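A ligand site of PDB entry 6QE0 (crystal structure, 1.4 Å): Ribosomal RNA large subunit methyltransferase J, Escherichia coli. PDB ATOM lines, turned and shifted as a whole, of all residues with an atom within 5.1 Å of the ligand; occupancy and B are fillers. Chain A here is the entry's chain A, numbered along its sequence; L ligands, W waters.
The backbone carbonyl oxygen (O) of His 45 sits at hydrogen-bond distance from a nitrogen (N1) of the ligand, 2.8 Å away. O of Pro 169 sits at hydrogen-bond distance from O1 of the ligand, at 2.4 Å. The side-chain carboxylate of Asp 18 is in hydrogen-bond range of an oxygen (O2) of the ligand, at 2.5 Å. The backbone NH (N) of Ser 103 lies within hydrogen-bond range of an oxygen (O8) of the ligand, 3.2 Å away. An oxygen (O9) of the ligand lies within salt-bridge range of the side-chain amino group (NZ) of Lys 21 (3.6 Å). The side-chain hydroxyl (OG) of Ser 103 sits at hydrogen-bond distance from a nitrogen (N1) of the ligand (2.9 Å). A nitrogen (N1) of the ligand is in salt-bridge range of the side-chain carboxylate (OD2) of Asp 167 (2.8 Å). The side-chain carboxylate (OD1) of Asp 43 is in salt-bridge range of a nitrogen (N1) of the ligand, at 3.5 Å. A ring nitrogen (NE2) of His 22 sits at hydrogen-bond distance from an oxygen (O9) of the ligand (2.8 Å).
The side-chain carboxylate (OD2) of Asp 18 is in hydrogen-bond range of the backbone NH (N) of Gly 14 (2.9 Å). The backbone NH (N) of Asp 18 sits at hydrogen-bond distance from the side-chain amide oxygen (OD1) of Asn 15 (3.0 Å). The backbone NH (N) of Ala 13 sits at hydrogen-bond distance from the side-chain hydroxyl (OG) of Ser 10 (3.1 Å). The side-chain hydroxyl (OH) of Tyr 170 sits at hydrogen-bond distance from the backbone carbonyl oxygen (O) of Trp 198. The backbone NH (N) of Ser 103 sits at hydrogen-bond distance from a ring nitrogen (NE2) of His 22, at 3.4 Å. The side-chain carboxylate of Asp 18 is in salt-bridge range of the side-chain amino group of Lys 21. The side-chain hydroxyl (OG) of Ser 103 lies within hydrogen-bond range of the side-chain carboxylate (OD2) of Asp 43, at 2.6 Å. The side-chain carboxylate (OD2) of Asp 167 lies within salt-bridge range of the side-chain amino group (NZ) of Lys 21, at 2.5 Å.
Residues that only touch the ligand: Ala 13, His 12, Gly 102, Met 238, Tyr 170, Ala 46, Tyr 51, Pro 200, Glu 171, Gly 47, Leu 165 and Trp 198. Hydrophobic or aromatic side chains that line the ligand: His 12, Ala 13, His 22, Leu 165, Pro 169, Tyr 170, Trp 198, Pro 200 and Met 238. Along chain A the residues within 4 Å of the ligand span positions 12 to 238.
Water W1 bridges the side-chain hydroxyl of Ser 10 (2.7 Å) and a nitrogen (N12) of the ligand (2.9 Å). Water W2 lies within hydrogen-bond range of the backbone carbonyl oxygen (O) of Ala 46 (2.5 Å), an oxygen (O8) of the ligand (2.9 Å) and the side-chain hydroxyl (OH) of Tyr 51 (3.0 Å). Water W5 bridges an oxygen (O5) of the ligand (2.9 Å) and the backbone carbonyl oxygen (O) of Tyr 170 (3.1 Å). Water W6 bridges OD1 of Asp 18 (3.1 Å) and OD1 of Asn 15 (3.3 Å).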
ATOM      1  N   SER A  10      -4.706   8.693  26.959  1.00  0.00           N
ATOM      2  CA  SER A  10      -5.213   7.933  25.824  1.00  0.00           C
ATOM      3  C   SER A  10      -5.676   6.565  26.283  1.00  0.00           C
ATOM      4  O   SER A  10      -4.988   5.911  27.074  1.00  0.00           O
ATOM      5  CB  SER A  10      -4.140   7.767  24.741  1.00  0.00           C
ATOM      6  OG  SER A  10      -4.638   6.973  23.671  1.00  0.00           O
ATOM      7  N   HIS A  12      -6.182   4.239  23.929  1.00  0.00           N
ATOM      8  CA  HIS A  12      -5.704   3.372  22.863  1.00  0.00           C
ATOM      9  C   HIS A  12      -4.185   3.227  22.836  1.00  0.00           C
ATOM     10  O   HIS A  12      -3.688   2.250  22.272  1.00  0.00           O
ATOM     11  CB  HIS A  12      -6.141   3.933  21.520  1.00  0.00           C
ATOM     12  CG  HIS A  12      -7.607   4.188  21.429  1.00  0.00           C
ATOM     13  ND1 HIS A  12      -8.190   5.368  21.855  1.00  0.00           N
ATOM     14  CD2 HIS A  12      -8.629   3.409  20.980  1.00  0.00           C
ATOM     15  CE1 HIS A  12      -9.501   5.303  21.663  1.00  0.00           C
ATOM     16  NE2 HIS A  12      -9.784   4.123  21.136  1.00  0.00           N
ATOM     17  N   ALA A  13      -3.451   4.161  23.421  1.00  0.00           N
ATOM     18  CA  ALA A  13      -2.005   4.205  23.230  1.00  0.00           C
ATOM     19  C   ALA A  13      -1.366   2.914  23.735  1.00  0.00           C
ATOM     20  O   ALA A  13      -1.771   2.365  24.766  1.00  0.00           O
ATOM     21  CB  ALA A  13      -1.439   5.404  23.981  1.00  0.00           C
ATOM     22  N   GLY A  14      -0.370   2.428  22.986  1.00  0.00           N
ATOM     23  CA  GLY A  14       0.288   1.175  23.314  1.00  0.00           C
ATOM     24  C   GLY A  14      -0.490  -0.067  22.961  1.00  0.00           C
ATOM     25  O   GLY A  14      -0.132  -1.151  23.418  1.00  0.00           O
ATOM     26  N   ASN A  15      -1.504   0.061  22.120  1.00  0.00           N
ATOM     27  CA  ASN A  15      -2.245  -1.123  21.693  1.00  0.00           C
ATOM     28  C   ASN A  15      -1.443  -1.913  20.672  1.00  0.00           C
ATOM     29  O   ASN A  15      -0.307  -1.580  20.331  1.00  0.00           O
ATOM     30  CB  ASN A  15      -3.622  -0.725  21.141  1.00  0.00           C
ATOM     31  CG  ASN A  15      -3.520   0.031  19.826  1.00  0.00           C
ATOM     32  OD1 ASN A  15      -2.469   0.531  19.452  1.00  0.00           O
ATOM     33  ND2 ASN A  15      -4.650   0.137  19.140  1.00  0.00           N
ATOM     34  N   ASP A  18      -0.078   0.166  17.752  1.00  0.00           N
ATOM     35  CA  ASP A  18       1.076   0.998  18.112  1.00  0.00           C
ATOM     36  C   ASP A  18       2.330   0.137  18.218  1.00  0.00           C
ATOM     37  O   ASP A  18       3.412   0.519  17.747  1.00  0.00           O
ATOM     38  CB  ASP A  18       0.788   1.692  19.454  1.00  0.00           C
ATOM     39  CG  ASP A  18      -0.056   2.963  19.320  1.00  0.00           C
ATOM     40  OD1 ASP A  18      -0.436   3.344  18.189  1.00  0.00           O
ATOM     41  OD2 ASP A  18      -0.368   3.579  20.352  1.00  0.00           O
ATOM     42  N   LYS A  21       3.415  -0.546  14.699  1.00  0.00           N
ATOM     43  CA  LYS A  21       3.819   0.650  13.952  1.00  0.00           C
ATOM     44  C   LYS A  21       5.140   1.217  14.463  1.00  0.00           C
ATOM     45  O   LYS A  21       6.043   1.527  13.664  1.00  0.00           O
ATOM     46  CB  LYS A  21       2.679   1.673  14.062  1.00  0.00           C
ATOM     47  CG  LYS A  21       3.114   3.080  13.682  1.00  0.00           C
ATOM     48  CD  LYS A  21       1.932   4.043  13.622  1.00  0.00           C
ATOM     49  CE  LYS A  21       1.133   4.072  14.921  1.00  0.00           C
ATOM     50  NZ  LYS A  21      -0.095   4.931  14.788  1.00  0.00           N
ATOM     51  N   HIS A  22       5.289   1.296  15.778  1.00  0.00           N
ATOM     52  CA  HIS A  22       6.504   1.869  16.363  1.00  0.00           C
ATOM     53  C   HIS A  22       7.675   0.904  16.284  1.00  0.00           C
ATOM     54  O   HIS A  22       8.838   1.336  16.194  1.00  0.00           O
ATOM     55  CB  HIS A  22       6.182   2.352  17.782  1.00  0.00           C
ATOM     56  CG  HIS A  22       5.160   3.446  17.807  1.00  0.00           C
ATOM     57  ND1 HIS A  22       4.174   3.547  18.765  1.00  0.00           N
ATOM     58  CD2 HIS A  22       4.956   4.469  16.940  1.00  0.00           C
ATOM     59  CE1 HIS A  22       3.414   4.605  18.499  1.00  0.00           C
ATOM     60  NE2 HIS A  22       3.867   5.183  17.404  1.00  0.00           N
ATOM     61  N   ASP A  43       7.009  13.440  10.194  1.00  0.00           N
ATOM     62  CA  ASP A  43       5.846  12.805  10.842  1.00  0.00           C
ATOM     63  C   ASP A  43       4.644  13.655  10.452  1.00  0.00           C
ATOM     64  O   ASP A  43       4.446  14.746  11.004  1.00  0.00           O
ATOM     65  CB  ASP A  43       6.046  12.829  12.340  1.00  0.00           C
ATOM     66  CG  ASP A  43       5.216  11.796  13.079  1.00  0.00           C
ATOM     67  OD1 ASP A  43       4.118  11.462  12.592  1.00  0.00           O
ATOM     68  OD2 ASP A  43       5.659  11.340  14.170  1.00  0.00           O
ATOM     69  N   HIS A  45       1.285  13.196  10.743  1.00  0.00           N
ATOM     70  CA  HIS A  45       0.251  13.311  11.764  1.00  0.00           C
ATOM     71  C   HIS A  45       0.839  12.820  13.081  1.00  0.00           C
ATOM     72  O   HIS A  45       0.698  11.657  13.462  1.00  0.00           O
ATOM     73  CB  HIS A  45      -0.967  12.498  11.322  1.00  0.00           C
ATOM     74  CG  HIS A  45      -1.558  12.965  10.022  1.00  0.00           C
ATOM     75  ND1 HIS A  45      -1.000  12.672   8.791  1.00  0.00           N
ATOM     76  CD2 HIS A  45      -2.649  13.733   9.761  1.00  0.00           C
ATOM     77  CE1 HIS A  45      -1.725  13.232   7.841  1.00  0.00           C
ATOM     78  NE2 HIS A  45      -2.727  13.872   8.405  1.00  0.00           N
ATOM     79  N   ALA A  46       1.498  13.730  13.796  1.00  0.00           N
ATOM     80  CA  ALA A  46       2.398  13.363  14.878  1.00  0.00           C
ATOM     81  C   ALA A  46       1.718  13.156  16.236  1.00  0.00           C
ATOM     82  O   ALA A  46       2.331  12.566  17.132  1.00  0.00           O
ATOM     83  CB  ALA A  46       3.472  14.448  15.044  1.00  0.00           C
ATOM     84  N   GLY A  47       0.496  13.645  16.414  1.00  0.00           N
ATOM     85  CA  GLY A  47      -0.114  13.461  17.714  1.00  0.00           C
ATOM     86  C   GLY A  47       0.472  14.367  18.788  1.00  0.00           C
ATOM     87  O   GLY A  47       1.079  15.408  18.515  1.00  0.00           O
ATOM     88  N   TYR A  51       1.664   9.756  25.700  1.00  0.00           N
ATOM     89  CA  TYR A  51       0.324   9.597  26.240  1.00  0.00           C
ATOM     90  C   TYR A  51       0.407   8.985  27.619  1.00  0.00           C
ATOM     91  O   TYR A  51       1.184   8.056  27.851  1.00  0.00           O
ATOM     92  CB  TYR A  51      -0.551   8.715  25.330  1.00  0.00           C
ATOM     93  CG  TYR A  51      -0.642   9.320  23.951  1.00  0.00           C
ATOM     94  CD1 TYR A  51      -1.511  10.366  23.689  1.00  0.00           C
ATOM     95  CD2 TYR A  51       0.225   8.910  22.935  1.00  0.00           C
ATOM     96  CE1 TYR A  51      -1.568  10.960  22.436  1.00  0.00           C
ATOM     97  CE2 TYR A  51       0.182   9.503  21.684  1.00  0.00           C
ATOM     98  CZ  TYR A  51      -0.712  10.518  21.438  1.00  0.00           C
ATOM     99  OH  TYR A  51      -0.772  11.101  20.198  1.00  0.00           O
ATOM    100  N   GLY A 102       4.741   8.206  21.754  1.00  0.00           N
ATOM    101  CA  GLY A 102       4.282   8.231  20.385  1.00  0.00           C
ATOM    102  C   GLY A 102       5.435   8.302  19.405  1.00  0.00           C
ATOM    103  O   GLY A 102       6.608   8.419  19.769  1.00  0.00           O
ATOM    104  N   SER A 103       5.087   8.240  18.124  1.00  0.00           N
ATOM    105  CA  SER A 103       6.090   8.291  17.060  1.00  0.00           C
ATOM    106  C   SER A 103       7.051   9.466  17.148  1.00  0.00           C
ATOM    107  O   SER A 103       8.234   9.280  16.831  1.00  0.00           O
ATOM    108  CB  SER A 103       5.445   8.190  15.664  1.00  0.00           C
ATOM    109  OG  SER A 103       4.626   9.313  15.378  1.00  0.00           O
ATOM    110  N   PRO A 104       6.638  10.679  17.552  1.00  0.00           N
ATOM    111  CA  PRO A 104       7.635  11.767  17.630  1.00  0.00           C
ATOM    112  C   PRO A 104       8.700  11.529  18.693  1.00  0.00           C
ATOM    113  O   PRO A 104       9.853  11.947  18.499  1.00  0.00           O
ATOM    114  CB  PRO A 104       6.781  13.002  17.939  1.00  0.00           C
ATOM    115  CG  PRO A 104       5.388  12.626  17.486  1.00  0.00           C
ATOM    116  CD  PRO A 104       5.290  11.184  17.831  1.00  0.00           C
ATOM    117  N   ASP A 126      -3.599  18.609  21.173  1.00  0.00           N
ATOM    118  CA  ASP A 126      -2.414  17.779  21.078  1.00  0.00           C
ATOM    119  C   ASP A 126      -1.216  18.569  20.570  1.00  0.00           C
ATOM    120  O   ASP A 126      -0.079  18.290  20.959  1.00  0.00           O
ATOM    121  CB  ASP A 126      -2.644  16.589  20.140  1.00  0.00           C
ATOM    122  CG  ASP A 126      -3.478  15.476  20.775  1.00  0.00           C
ATOM    123  OD1 ASP A 126      -3.696  15.492  22.001  1.00  0.00           O
ATOM    124  OD2 ASP A 126      -3.909  14.578  20.033  1.00  0.00           O
ATOM    125  N   LEU A 165       6.824   9.142   7.908  1.00  0.00           N
ATOM    126  CA  LEU A 165       5.756   8.367   8.529  1.00  0.00           C
ATOM    127  C   LEU A 165       4.424   9.056   8.238  1.00  0.00           C
ATOM    128  O   LEU A 165       4.236  10.223   8.590  1.00  0.00           O
ATOM    129  CB  LEU A 165       5.979   8.200  10.035  1.00  0.00           C
ATOM    130  CG  LEU A 165       4.824   7.424  10.736  1.00  0.00           C
ATOM    131  CD1 LEU A 165       4.765   5.940  10.317  1.00  0.00           C
ATOM    132  CD2 LEU A 165       4.872   7.529  12.247  1.00  0.00           C
ATOM    133  N   ASP A 167       0.459   8.674   8.981  1.00  0.00           N
ATOM    134  CA  ASP A 167      -0.258   7.954  10.049  1.00  0.00           C
ATOM    135  C   ASP A 167      -1.450   8.797  10.499  1.00  0.00           C
ATOM    136  O   ASP A 167      -1.515   9.252  11.654  1.00  0.00           O
ATOM    137  CB  ASP A 167       0.701   7.648  11.208  1.00  0.00           C
ATOM    138  CG  ASP A 167       0.076   6.871  12.311  1.00  0.00           C
ATOM    139  OD1 ASP A 167      -0.912   6.162  12.038  1.00  0.00           O
ATOM    140  OD2 ASP A 167       0.582   6.953  13.444  1.00  0.00           O
ATOM    141  N   PRO A 168      -2.408   9.037   9.603  1.00  0.00           N
ATOM    142  CA  PRO A 168      -3.548   9.930   9.931  1.00  0.00           C
ATOM    143  C   PRO A 168      -4.599   9.200  10.743  1.00  0.00           C
ATOM    144  O   PRO A 168      -4.494   7.983  10.951  1.00  0.00           O
ATOM    145  CB  PRO A 168      -4.080  10.292   8.535  1.00  0.00           C
ATOM    146  CG  PRO A 168      -3.842   9.057   7.746  1.00  0.00           C
ATOM    147  CD  PRO A 168      -2.548   8.462   8.257  1.00  0.00           C
ATOM    148  N   PRO A 169      -5.641   9.906  11.217  1.00  0.00           N
ATOM    149  CA  PRO A 169      -6.616   9.231  12.090  1.00  0.00           C
ATOM    150  C   PRO A 169      -7.527   8.271  11.365  1.00  0.00           C
ATOM    151  O   PRO A 169      -8.064   7.353  12.017  1.00  0.00           O
ATOM    152  CB  PRO A 169      -7.418  10.404  12.691  1.00  0.00           C
ATOM    153  CG  PRO A 169      -6.499  11.603  12.542  1.00  0.00           C
ATOM    154  CD  PRO A 169      -5.815  11.370  11.219  1.00  0.00           C
ATOM    155  N   TYR A 170      -7.729   8.435  10.065  1.00  0.00           N
ATOM    156  CA  TYR A 170      -8.768   7.725   9.329  1.00  0.00           C
ATOM    157  C   TYR A 170     -10.146   7.935   9.964  1.00  0.00           C
ATOM    158  O   TYR A 170     -10.992   7.044   9.950  1.00  0.00           O
ATOM    159  CB  TYR A 170      -8.451   6.247   9.134  1.00  0.00           C
ATOM    160  CG  TYR A 170      -7.172   5.953   8.358  1.00  0.00           C
ATOM    161  CD1 TYR A 170      -5.949   5.829   9.002  1.00  0.00           C
ATOM    162  CD2 TYR A 170      -7.194   5.770   6.970  1.00  0.00           C
ATOM    163  CE1 TYR A 170      -4.785   5.538   8.311  1.00  0.00           C
ATOM    164  CE2 TYR A 170      -6.034   5.481   6.256  1.00  0.00           C
ATOM    165  CZ  TYR A 170      -4.824   5.375   6.935  1.00  0.00           C
ATOM    166  OH  TYR A 170      -3.669   5.064   6.248  1.00  0.00           O
ATOM    167  N   GLU A 171     -10.349   9.110  10.554  1.00  0.00           N
ATOM    168  CA  GLU A 171     -11.701   9.511  10.958  1.00  0.00           C
ATOM    169  C   GLU A 171     -12.563   9.776   9.733  1.00  0.00           C
ATOM    170  O   GLU A 171     -13.745   9.415   9.704  1.00  0.00           O
ATOM    171  CB  GLU A 171     -11.629  10.792  11.788  1.00  0.00           C
ATOM    172  CG  GLU A 171     -11.735  10.600  13.275  1.00  0.00           C
ATOM    173  CD  GLU A 171     -12.428  11.777  13.947  1.00  0.00           C
ATOM    174  OE1 GLU A 171     -12.543  11.770  15.198  1.00  0.00           O
ATOM    175  OE2 GLU A 171     -12.856  12.705  13.227  1.00  0.00           O
ATOM    176  N   TRP A 198       0.856   3.795   7.952  1.00  0.00           N
ATOM    177  CA  TRP A 198       0.050   2.979   8.865  1.00  0.00           C
ATOM    178  C   TRP A 198      -1.397   3.011   8.408  1.00  0.00           C
ATOM    179  O   TRP A 198      -1.923   4.048   7.999  1.00  0.00           O
ATOM    180  CB  TRP A 198       0.129   3.479  10.296  1.00  0.00           C
ATOM    181  CG  TRP A 198      -0.693   2.590  11.206  1.00  0.00           C
ATOM    182  CD1 TRP A 198      -0.294   1.441  11.785  1.00  0.00           C
ATOM    183  CD2 TRP A 198      -2.064   2.782  11.573  1.00  0.00           C
ATOM    184  NE1 TRP A 198      -1.318   0.882  12.509  1.00  0.00           N
ATOM    185  CE2 TRP A 198      -2.417   1.704  12.410  1.00  0.00           C
ATOM    186  CE3 TRP A 198      -3.025   3.763  11.293  1.00  0.00           C
ATOM    187  CZ2 TRP A 198      -3.701   1.573  12.962  1.00  0.00           C
ATOM    188  CZ3 TRP A 198      -4.271   3.649  11.836  1.00  0.00           C
ATOM    189  CH2 TRP A 198      -4.598   2.555  12.650  1.00  0.00           C
ATOM    190  N   PRO A 200      -5.455   1.106   9.341  1.00  0.00           N
ATOM    191  CA  PRO A 200      -6.277   0.157  10.089  1.00  0.00           C
ATOM    192  C   PRO A 200      -7.088  -0.695   9.150  1.00  0.00           C
ATOM    193  O   PRO A 200      -7.460  -0.227   8.068  1.00  0.00           O
ATOM    194  CB  PRO A 200      -7.208   1.072  10.891  1.00  0.00           C
ATOM    195  CG  PRO A 200      -7.435   2.236   9.969  1.00  0.00           C
ATOM    196  CD  PRO A 200      -6.146   2.394   9.124  1.00  0.00           C
ATOM    197  N   VAL A 202     -10.592  -1.961   9.072  1.00  0.00           N
ATOM    198  CA  VAL A 202     -11.969  -2.040   9.549  1.00  0.00           C
ATOM    199  C   VAL A 202     -12.842  -2.811   8.565  1.00  0.00           C
ATOM    200  O   VAL A 202     -13.404  -3.849   8.909  1.00  0.00           O
ATOM    201  CB  VAL A 202     -12.552  -0.644   9.849  1.00  0.00           C
ATOM    202  CG1 VAL A 202     -13.966  -0.759  10.446  1.00  0.00           C
ATOM    203  CG2 VAL A 202     -11.619   0.146  10.785  1.00  0.00           C
ATOM    204  N   MET A 238     -11.749  -2.226  14.307  1.00  0.00           N
ATOM    205  CA  MET A 238     -10.438  -2.503  13.754  1.00  0.00           C
ATOM    206  C   MET A 238      -9.982  -3.898  14.182  1.00  0.00           C
ATOM    207  O   MET A 238      -9.663  -4.116  15.350  1.00  0.00           O
ATOM    208  CB  MET A 238      -9.428  -1.469  14.220  1.00  0.00           C
ATOM    209  CG  MET A 238      -8.022  -1.746  13.694  1.00  0.00           C
ATOM    210  SD  MET A 238      -6.848  -0.461  14.125  1.00  0.00           S
ATOM    211  CE  MET A 238      -6.586  -0.786  15.865  1.00  0.00           C
HETATM  212  O1  LIG L   1      -7.986   4.951  12.454  1.00  0.00           O
HETATM  213  O2  LIG L   1      -1.752   5.699  20.211  1.00  0.00           O
HETATM  214  C1  LIG L   1       1.329   9.400  15.636  1.00  0.00           C
HETATM  215  C2  LIG L   1      -0.175   9.269  15.472  1.00  0.00           C
HETATM  216  C3  LIG L   1      -0.996   9.887  16.688  1.00  0.00           C
HETATM  217  C4  LIG L   1      -3.333  10.644  17.256  1.00  0.00           C
HETATM  218  C5  LIG L   1      -4.825  10.196  17.410  1.00  0.00           C
HETATM  219  C6  LIG L   1      -7.048   9.769  16.106  1.00  0.00           C
HETATM  220  C7  LIG L   1      -7.027   8.389  15.660  1.00  0.00           C
HETATM  221  C8  LIG L   1      -6.560   6.365  15.007  1.00  0.00           C
HETATM  222  C9  LIG L   1      -8.904   5.375  14.757  1.00  0.00           C
HETATM  223  C10 LIG L   1      -8.949   3.003  15.164  1.00  0.00           C
HETATM  224  C11 LIG L   1      -7.639   2.626  15.930  1.00  0.00           C
HETATM  225  C12 LIG L   1      -8.697   3.123  13.851  1.00  0.00           C
HETATM  226  C13 LIG L   1      -7.992   4.497  13.793  1.00  0.00           C
HETATM  227  C14 LIG L   1      -8.217   7.704  15.471  1.00  0.00           C
HETATM  228  C15 LIG L   1      -9.384   9.594  16.114  1.00  0.00           C
HETATM  229  C16 LIG L   1      -2.890   8.193  16.598  1.00  0.00           C
HETATM  230  C17 LIG L   1      -2.447   7.523  17.974  1.00  0.00           C
HETATM  231  C18 LIG L   1      -3.953   6.567  19.587  1.00  0.00           C
HETATM  232  C19 LIG L   1      -2.786   5.593  19.214  1.00  0.00           C
HETATM  233  C20 LIG L   1      -2.366   6.153  17.864  1.00  0.00           C
HETATM  234  C21 LIG L   1      -5.561   5.061  18.361  1.00  0.00           C
HETATM  235  C22 LIG L   1      -7.427   6.160  18.595  1.00  0.00           C
HETATM  236  C23 LIG L   1      -8.695   6.734  18.645  1.00  0.00           C
HETATM  237  C24 LIG L   1      -7.847   8.537  19.860  1.00  0.00           C
HETATM  238  C25 LIG L   1      -6.389   6.877  19.222  1.00  0.00           C
HETATM  239  C26 LIG L   1       1.913   8.350  16.589  1.00  0.00           C
HETATM  240  N1  LIG L   1       1.960   9.272  14.305  1.00  0.00           N
HETATM  241  N2  LIG L   1      -2.483   9.653  16.451  1.00  0.00           N
HETATM  242  N3  LIG L   1      -5.781  10.551  16.321  1.00  0.00           N
HETATM  243  N4  LIG L   1      -6.029   7.523  15.362  1.00  0.00           N
HETATM  244  N5  LIG L   1      -7.887   6.460  15.040  1.00  0.00           N
HETATM  245  N6  LIG L   1      -9.396   8.316  15.706  1.00  0.00           N
HETATM  246  N7  LIG L   1      -8.237  10.283  16.304  1.00  0.00           N
HETATM  247  N8  LIG L   1      -5.267   6.185  19.054  1.00  0.00           N
HETATM  248  N9  LIG L   1      -6.868   5.042  18.071  1.00  0.00           N
HETATM  249  N10 LIG L   1      -9.860   6.073  18.052  1.00  0.00           N
HETATM  250  N11 LIG L   1      -8.864   7.906  19.284  1.00  0.00           N
HETATM  251  N12 LIG L   1      -6.626   8.048  19.840  1.00  0.00           N
HETATM  252  O3  LIG L   1      -9.399   4.491  15.618  1.00  0.00           O
HETATM  253  O4  LIG L   1      -7.957   2.477  17.250  1.00  0.00           O
HETATM  254  O5  LIG L   1      -9.934   3.163  13.112  1.00  0.00           O
HETATM  255  O6  LIG L   1      -3.595   7.761  19.086  1.00  0.00           O
HETATM  256  O7  LIG L   1      -1.093   5.713  17.532  1.00  0.00           O
HETATM  257  O8  LIG L   1       1.941   8.592  17.876  1.00  0.00           O
HETATM  258  O9  LIG L   1       2.374   7.226  16.124  1.00  0.00           O
HETATM  259  O   HOH W   1      -4.978   9.035  21.955  1.00  0.00           O
HETATM  260  O   HOH W   2       2.041  11.145  19.224  1.00  0.00           O
HETATM  261  O   HOH W   3      -9.569  11.705  18.800  1.00  0.00           O
HETATM  262  O   HOH W   4      -2.965  10.391  13.737  1.00  0.00           O
HETATM  263  O   HOH W   5     -11.188   4.054  10.629  1.00  0.00           O
HETATM  264  O   HOH W   6      -3.260   2.802  17.129  1.00  0.00           O
HETATM  265  O   HOH W   7     -11.000   9.610  19.503  1.00  0.00           O
HETATM  266  O   HOH W   8      -3.878  13.860  17.152  1.00  0.00           O
HETATM  267  O   HOH W   9     -12.429   1.721  14.408  1.00  0.00           O
HETATM  268  O   HOH W  10       1.291   6.574  19.583  1.00  0.00           O
HETATM  269  O   HOH W  11      -6.733  13.297  16.453  1.00  0.00           O
